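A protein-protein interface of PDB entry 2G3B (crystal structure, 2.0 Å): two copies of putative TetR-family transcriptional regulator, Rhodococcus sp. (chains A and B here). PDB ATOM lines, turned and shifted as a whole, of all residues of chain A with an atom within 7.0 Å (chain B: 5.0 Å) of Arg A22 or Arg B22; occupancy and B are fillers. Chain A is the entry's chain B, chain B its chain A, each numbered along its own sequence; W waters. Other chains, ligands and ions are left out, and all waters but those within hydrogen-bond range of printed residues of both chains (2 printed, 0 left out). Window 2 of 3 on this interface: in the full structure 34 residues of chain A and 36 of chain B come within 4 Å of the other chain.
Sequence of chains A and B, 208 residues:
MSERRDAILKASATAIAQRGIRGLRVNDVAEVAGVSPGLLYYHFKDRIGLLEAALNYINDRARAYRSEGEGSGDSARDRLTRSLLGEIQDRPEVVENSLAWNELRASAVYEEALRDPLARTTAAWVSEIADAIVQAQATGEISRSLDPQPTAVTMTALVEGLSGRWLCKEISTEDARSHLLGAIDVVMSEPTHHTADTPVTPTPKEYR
NE of Arg A22 is in hydrogen-bond range of O of Arg B19.
NE of Arg B22 is in hydrogen-bond range of O of Arg A22 (3.5 Å).
NH2 of Arg A22 is in salt-bridge range of OE2 of Glu B103 (2.5 Å).
The backbone carbonyl oxygen (O) of Gly B23 sits at hydrogen-bond distance from the guanidinium group (NH1) of Arg B19 (3.5 Å).
The side-chain hydroxyl (OH) of Tyr A110 lies within hydrogen-bond range of the backbone NH (N) of Arg A22, at 3.2 Å.
Among the printed residues, pairs that only touch across the chains: Arg A22 with Gln B18 (3.9 Å), Tyr A110 with Glu B103 (3.9 Å) and Arg A22 with Gly B20 (3.9 Å).
Of chain B, only Gln B18 (3.9 Å), Arg B19 (3.4 Å), Gly B20 (3.9 Å), Arg B22 (3.5 Å) and Glu B103 (2.5 Å) come within 4 Å of Arg A22.
Printed residues of chain A within 4 Å of Gln B18: Arg A22.
Of the printed residues of chain A, Arg B19 touches Arg A22 (3.4 Å).
Printed residues of chain A within 4 Å of Gly B20: Arg A22.
Of the printed residues of chain A, Glu B103 touches Arg A22 and Tyr A110.
The nearest printed residue of chain B that does not touch Arg A22 is Gly B23 (5.7 Å).
The nearest residue of chain A that does not touch Arg B22 is Gly A23 (4.3 Å).
The nearest printed residue of chain B that does not touch Tyr A110 is Gln B18 (6.0 Å).
Of the 8 printed residues of chain B, 5 touch a printed residue of chain A.
Printed residues of chain B that touch a printed residue of chain A: Gln B18, Arg B19, Gly B20, Arg B22 and Glu B103.
Among the printed residues, 6 pairs touch across the chains.
Among the printed residues, Asp or Glu carboxylates within 4 Å of a Lys or Arg side-chain nitrogen of the other chain: Arg A22 with Glu B103.
Arg A22 touches Arg B19, but with the chains exchanged Arg A19 does not touch Arg B22 (5.8 Å).
Arg A22 touches Gly B20, but with the chains exchanged Gly A20 does not touch Arg B22 (6.9 Å).
Arg A22 touches its own counterpart, Arg B22.
Arg A22 touches Glu B103, but with the chains exchanged Glu A103 does not touch Arg B22 (7.7 Å).
Of the 6 pairs that touch across the chains among the printed residues, 1 has its exchanged pair printed and touching as well.
Water W1 lies within hydrogen-bond range of NE of Arg A22 and OE1 of Glu B103.
Water W2 lies within hydrogen-bond range of the backbone carbonyl oxygen of Ala A106 (2.5 Å) and the side-chain carboxylate of Glu B103 (3.3 Å).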
ATOM      1  N   ARG A  19      26.865  -2.237  10.673  1.00  0.00           N
ATOM      2  CA  ARG A  19      27.823  -1.148  10.541  1.00  0.00           C
ATOM      3  C   ARG A  19      27.448  -0.337   9.333  1.00  0.00           C
ATOM      4  O   ARG A  19      27.742   0.872   9.252  1.00  0.00           O
ATOM      5  CB  ARG A  19      29.218  -1.712  10.326  1.00  0.00           C
ATOM      6  CG  ARG A  19      29.962  -2.171  11.592  1.00  0.00           C
ATOM      7  CD  ARG A  19      30.736  -3.487  11.378  1.00  0.00           C
ATOM      8  NE  ARG A  19      31.481  -3.928  12.568  1.00  0.00           N
ATOM      9  CZ  ARG A  19      31.231  -5.021  13.307  1.00  0.00           C
ATOM     10  NH1 ARG A  19      30.225  -5.850  13.019  1.00  0.00           N
ATOM     11  NH2 ARG A  19      32.001  -5.283  14.361  1.00  0.00           N
ATOM     12  N   GLY A  20      26.784  -0.996   8.376  1.00  0.00           N
ATOM     13  CA  GLY A  20      26.505  -0.331   7.129  1.00  0.00           C
ATOM     14  C   GLY A  20      27.739  -0.418   6.248  1.00  0.00           C
ATOM     15  O   GLY A  20      28.845  -0.738   6.708  1.00  0.00           O
ATOM     16  N   ILE A  21      27.528  -0.161   4.965  1.00  0.00           N
ATOM     17  CA  ILE A  21      28.562  -0.365   3.957  1.00  0.00           C
ATOM     18  C   ILE A  21      29.485   0.814   3.862  1.00  0.00           C
ATOM     19  O   ILE A  21      30.675   0.650   3.605  1.00  0.00           O
ATOM     20  CB  ILE A  21      27.953  -0.658   2.530  1.00  0.00           C
ATOM     21  CG1 ILE A  21      27.462  -2.084   2.493  1.00  0.00           C
ATOM     22  CG2 ILE A  21      29.027  -0.365   1.366  1.00  0.00           C
ATOM     23  CD1 ILE A  21      28.489  -2.992   2.145  1.00  0.00           C
ATOM     24  N   ARG A  22      28.944   2.009   4.039  1.00  0.00           N
ATOM     25  CA  ARG A  22      29.774   3.181   3.902  1.00  0.00           C
ATOM     26  C   ARG A  22      30.928   3.192   4.947  1.00  0.00           C
ATOM     27  O   ARG A  22      30.728   2.949   6.158  1.00  0.00           O
ATOM     28  CB  ARG A  22      28.901   4.482   3.848  1.00  0.00           C
ATOM     29  CG  ARG A  22      29.617   5.660   3.138  1.00  0.00           C
ATOM     30  CD  ARG A  22      28.887   6.997   3.354  1.00  0.00           C
ATOM     31  NE  ARG A  22      27.526   7.080   2.789  1.00  0.00           N
ATOM     32  CZ  ARG A  22      27.253   7.595   1.600  1.00  0.00           C
ATOM     33  NH1 ARG A  22      28.248   8.030   0.831  1.00  0.00           N
ATOM     34  NH2 ARG A  22      26.004   7.695   1.181  1.00  0.00           N
ATOM     35  N   GLY A  23      32.159   3.404   4.481  1.00  0.00           N
ATOM     36  CA  GLY A  23      33.327   3.277   5.371  1.00  0.00           C
ATOM     37  C   GLY A  23      33.604   1.886   5.961  1.00  0.00           C
ATOM     38  O   GLY A  23      34.451   1.735   6.871  1.00  0.00           O
ATOM     39  N   LEU A  24      32.911   0.852   5.458  1.00  0.00           N
ATOM     40  CA  LEU A  24      33.297  -0.509   5.804  1.00  0.00           C
ATOM     41  C   LEU A  24      34.535  -0.878   5.029  1.00  0.00           C
ATOM     42  O   LEU A  24      34.529  -0.783   3.813  1.00  0.00           O
ATOM     43  CB  LEU A  24      32.206  -1.511   5.432  1.00  0.00           C
ATOM     44  CG  LEU A  24      32.338  -2.975   5.897  1.00  0.00           C
ATOM     45  CD1 LEU A  24      32.337  -3.148   7.431  1.00  0.00           C
ATOM     46  CD2 LEU A  24      31.233  -3.853   5.247  1.00  0.00           C
ATOM     47  N   ARG A  25      35.562  -1.375   5.710  1.00  0.00           N
ATOM     48  CA  ARG A  25      36.759  -1.785   5.000  1.00  0.00           C
ATOM     49  C   ARG A  25      37.091  -3.252   5.160  1.00  0.00           C
ATOM     50  O   ARG A  25      36.574  -3.918   6.062  1.00  0.00           O
ATOM     51  CB  ARG A  25      37.956  -0.896   5.344  1.00  0.00           C
ATOM     52  CG  ARG A  25      38.943  -0.753   4.149  1.00  0.00           C
ATOM     53  CD  ARG A  25      38.328  -1.212   2.783  1.00  0.00           C
ATOM     54  NE  ARG A  25      39.190  -2.131   2.031  1.00  0.00           N
ATOM     55  CZ  ARG A  25      39.922  -1.799   0.966  1.00  0.00           C
ATOM     56  NH1 ARG A  25      39.851  -0.584   0.495  1.00  0.00           N
ATOM     57  NH2 ARG A  25      40.665  -2.701   0.328  1.00  0.00           N
ATOM     58  N   ARG A  47      37.906  -5.265  -2.351  1.00  0.00           N
ATOM     59  CA  ARG A  47      36.719  -4.920  -1.564  1.00  0.00           C
ATOM     60  C   ARG A  47      35.414  -5.131  -2.324  1.00  0.00           C
ATOM     61  O   ARG A  47      34.437  -5.671  -1.763  1.00  0.00           O
ATOM     62  CB  ARG A  47      36.807  -3.500  -0.961  1.00  0.00           C
ATOM     63  CG  ARG A  47      35.541  -3.089  -0.143  1.00  0.00           C
ATOM     64  CD  ARG A  47      35.628  -1.612   0.255  1.00  0.00           C
ATOM     65  NE  ARG A  47      34.488  -1.101   1.026  1.00  0.00           N
ATOM     66  CZ  ARG A  47      33.457  -0.427   0.498  1.00  0.00           C
ATOM     67  NH1 ARG A  47      33.373  -0.221  -0.808  1.00  0.00           N
ATOM     68  NH2 ARG A  47      32.494   0.028   1.279  1.00  0.00           N
ATOM     69  N   GLU A 103      20.691  -3.081   3.548  1.00  0.00           N
ATOM     70  CA  GLU A 103      21.864  -2.187   3.450  1.00  0.00           C
ATOM     71  C   GLU A 103      22.548  -2.218   2.069  1.00  0.00           C
ATOM     72  O   GLU A 103      23.013  -1.230   1.612  1.00  0.00           O
ATOM     73  CB  GLU A 103      22.883  -2.537   4.552  1.00  0.00           C
ATOM     74  CG  GLU A 103      24.190  -1.759   4.423  1.00  0.00           C
ATOM     75  CD  GLU A 103      24.043  -0.220   4.645  1.00  0.00           C
ATOM     76  OE1 GLU A 103      23.014   0.223   5.185  1.00  0.00           O
ATOM     77  OE2 GLU A 103      25.021   0.508   4.343  1.00  0.00           O
ATOM     78  N   ALA A 106      20.506  -0.007  -0.169  1.00  0.00           N
ATOM     79  CA  ALA A 106      20.861   1.354   0.148  1.00  0.00           C
ATOM     80  C   ALA A 106      22.255   1.769  -0.398  1.00  0.00           C
ATOM     81  O   ALA A 106      22.432   2.918  -0.841  1.00  0.00           O
ATOM     82  CB  ALA A 106      20.838   1.559   1.682  1.00  0.00           C
ATOM     83  N   SER A 107      23.245   0.859  -0.310  1.00  0.00           N
ATOM     84  CA  SER A 107      24.649   1.237  -0.635  1.00  0.00           C
ATOM     85  C   SER A 107      24.897   1.454  -2.128  1.00  0.00           C
ATOM     86  O   SER A 107      25.784   2.247  -2.529  1.00  0.00           O
ATOM     87  CB  SER A 107      25.600   0.146  -0.105  1.00  0.00           C
ATOM     88  OG  SER A 107      25.543  -0.991  -0.995  1.00  0.00           O
ATOM     89  N   VAL A 109      23.310   2.961  -4.273  1.00  0.00           N
ATOM     90  CA  VAL A 109      23.189   4.347  -4.695  1.00  0.00           C
ATOM     91  C   VAL A 109      24.596   4.952  -4.916  1.00  0.00           C
ATOM     92  O   VAL A 109      24.826   5.621  -5.902  1.00  0.00           O
ATOM     93  CB  VAL A 109      22.401   5.186  -3.674  1.00  0.00           C
ATOM     94  CG1 VAL A 109      22.428   6.721  -4.060  1.00  0.00           C
ATOM     95  CG2 VAL A 109      20.953   4.659  -3.571  1.00  0.00           C
ATOM     96  N   TYR A 110      25.527   4.724  -3.985  1.00  0.00           N
ATOM     97  CA  TYR A 110      26.878   5.269  -4.111  1.00  0.00           C
ATOM     98  C   TYR A 110      27.952   4.229  -4.456  1.00  0.00           C
ATOM     99  O   TYR A 110      29.024   4.589  -4.915  1.00  0.00           O
ATOM    100  CB  TYR A 110      27.274   6.072  -2.846  1.00  0.00           C
ATOM    101  CG  TYR A 110      27.197   5.238  -1.611  1.00  0.00           C
ATOM    102  CD1 TYR A 110      28.275   4.431  -1.214  1.00  0.00           C
ATOM    103  CD2 TYR A 110      26.016   5.205  -0.860  1.00  0.00           C
ATOM    104  CE1 TYR A 110      28.161   3.611  -0.084  1.00  0.00           C
ATOM    105  CE2 TYR A 110      25.907   4.436   0.268  1.00  0.00           C
ATOM    106  CZ  TYR A 110      26.958   3.628   0.645  1.00  0.00           C
ATOM    107  OH  TYR A 110      26.785   2.834   1.758  1.00  0.00           O
ATOM    108  N   GLU A 111      27.690   2.943  -4.240  1.00  0.00           N
ATOM    109  CA  GLU A 111      28.659   1.902  -4.627  1.00  0.00           C
ATOM    110  C   GLU A 111      28.264   1.396  -5.975  1.00  0.00           C
ATOM    111  O   GLU A 111      27.597   0.351  -6.068  1.00  0.00           O
ATOM    112  CB  GLU A 111      28.621   0.712  -3.681  1.00  0.00           C
ATOM    113  CG  GLU A 111      29.280   0.921  -2.389  1.00  0.00           C
ATOM    114  CD  GLU A 111      30.790   1.093  -2.486  1.00  0.00           C
ATOM    115  OE1 GLU A 111      31.433   0.804  -3.539  1.00  0.00           O
ATOM    116  OE2 GLU A 111      31.320   1.507  -1.453  1.00  0.00           O
ATOM    117  N   GLN B  18      24.487  13.424   0.064  1.00  0.00           N
ATOM    118  CA  GLN B  18      25.739  13.212  -0.642  1.00  0.00           C
ATOM    119  C   GLN B  18      26.728  12.328   0.106  1.00  0.00           C
ATOM    120  O   GLN B  18      27.499  11.589  -0.531  1.00  0.00           O
ATOM    121  CB  GLN B  18      26.426  14.584  -0.900  1.00  0.00           C
ATOM    122  CG  GLN B  18      25.682  15.425  -1.974  1.00  0.00           C
ATOM    123  CD  GLN B  18      25.533  14.704  -3.330  1.00  0.00           C
ATOM    124  OE1 GLN B  18      24.414  14.381  -3.788  1.00  0.00           O
ATOM    125  NE2 GLN B  18      26.669  14.453  -3.982  1.00  0.00           N
ATOM    126  N   ARG B  19      26.724  12.434   1.428  1.00  0.00           N
ATOM    127  CA  ARG B  19      27.782  11.864   2.283  1.00  0.00           C
ATOM    128  C   ARG B  19      27.191  10.924   3.352  1.00  0.00           C
ATOM    129  O   ARG B  19      27.912  10.237   4.076  1.00  0.00           O
ATOM    130  CB  ARG B  19      28.558  13.007   2.952  1.00  0.00           C
ATOM    131  CG  ARG B  19      29.440  13.884   1.999  1.00  0.00           C
ATOM    132  CD  ARG B  19      30.260  14.952   2.808  1.00  0.00           C
ATOM    133  NE  ARG B  19      29.499  16.193   3.065  1.00  0.00           N
ATOM    134  CZ  ARG B  19      29.913  17.225   3.818  1.00  0.00           C
ATOM    135  NH1 ARG B  19      31.118  17.216   4.428  1.00  0.00           N
ATOM    136  NH2 ARG B  19      29.118  18.296   3.972  1.00  0.00           N
ATOM    137  N   GLY B  20      25.868  10.887   3.408  1.00  0.00           N
ATOM    138  CA  GLY B  20      25.125  10.110   4.372  1.00  0.00           C
ATOM    139  C   GLY B  20      25.187  10.727   5.759  1.00  0.00           C
ATOM    140  O   GLY B  20      25.862  11.722   5.988  1.00  0.00           O
ATOM    141  N   ILE B  21      24.499  10.089   6.698  1.00  0.00           N
ATOM    142  CA  ILE B  21      24.548  10.476   8.109  1.00  0.00           C
ATOM    143  C   ILE B  21      25.991  10.545   8.688  1.00  0.00           C
ATOM    144  O   ILE B  21      26.309  11.475   9.405  1.00  0.00           O
ATOM    145  CB  ILE B  21      23.490   9.587   8.884  1.00  0.00           C
ATOM    146  CG1 ILE B  21      22.067  10.069   8.574  1.00  0.00           C
ATOM    147  CG2 ILE B  21      23.750   9.359  10.351  1.00  0.00           C
ATOM    148  CD1 ILE B  21      21.942  11.557   8.359  1.00  0.00           C
ATOM    149  N   ARG B  22      26.868   9.595   8.359  1.00  0.00           N
ATOM    150  CA  ARG B  22      28.278   9.662   8.839  1.00  0.00           C
ATOM    151  C   ARG B  22      29.109  10.797   8.215  1.00  0.00           C
ATOM    152  O   ARG B  22      30.154  11.210   8.761  1.00  0.00           O
ATOM    153  CB  ARG B  22      28.998   8.342   8.604  1.00  0.00           C
ATOM    154  CG  ARG B  22      28.943   7.861   7.160  1.00  0.00           C
ATOM    155  CD  ARG B  22      29.158   6.353   7.065  1.00  0.00           C
ATOM    156  NE  ARG B  22      30.220   5.898   7.958  1.00  0.00           N
ATOM    157  CZ  ARG B  22      31.491   6.282   7.856  1.00  0.00           C
ATOM    158  NH1 ARG B  22      31.841   7.143   6.898  1.00  0.00           N
ATOM    159  NH2 ARG B  22      32.401   5.811   8.714  1.00  0.00           N
ATOM    160  N   GLY B  23      28.653  11.306   7.071  1.00  0.00           N
ATOM    161  CA  GLY B  23      29.420  12.343   6.375  1.00  0.00           C
ATOM    162  C   GLY B  23      28.960  13.738   6.716  1.00  0.00           C
ATOM    163  O   GLY B  23      29.588  14.729   6.278  1.00  0.00           O
ATOM    164  N   LEU B  24      27.861  13.802   7.481  1.00  0.00           N
ATOM    165  CA  LEU B  24      27.300  15.032   8.023  1.00  0.00           C
ATOM    166  C   LEU B  24      28.128  15.479   9.224  1.00  0.00           C
ATOM    167  O   LEU B  24      28.179  14.788  10.256  1.00  0.00           O
ATOM    168  CB  LEU B  24      25.862  14.809   8.487  1.00  0.00           C
ATOM    169  CG  LEU B  24      25.088  15.944   9.166  1.00  0.00           C
ATOM    170  CD1 LEU B  24      24.464  16.902   8.151  1.00  0.00           C
ATOM    171  CD2 LEU B  24      23.952  15.366  10.045  1.00  0.00           C
ATOM    172  N   GLU B 103      18.890   7.659   2.553  1.00  0.00           N
ATOM    173  CA  GLU B 103      19.970   7.556   3.562  1.00  0.00           C
ATOM    174  C   GLU B 103      19.447   7.449   4.986  1.00  0.00           C
ATOM    175  O   GLU B 103      19.866   6.595   5.759  1.00  0.00           O
ATOM    176  CB  GLU B 103      20.930   8.764   3.482  1.00  0.00           C
ATOM    177  CG  GLU B 103      21.853   8.726   2.262  1.00  0.00           C
ATOM    178  CD  GLU B 103      22.970   7.681   2.404  1.00  0.00           C
ATOM    179  OE1 GLU B 103      23.265   7.208   3.539  1.00  0.00           O
ATOM    180  OE2 GLU B 103      23.582   7.365   1.354  1.00  0.00           O
HETATM  181  O   HOH W   1      25.818   5.938   4.093  1.00  0.00           O
HETATM  182  O   HOH W   2      21.527   5.058   0.173  1.00  0.00           O
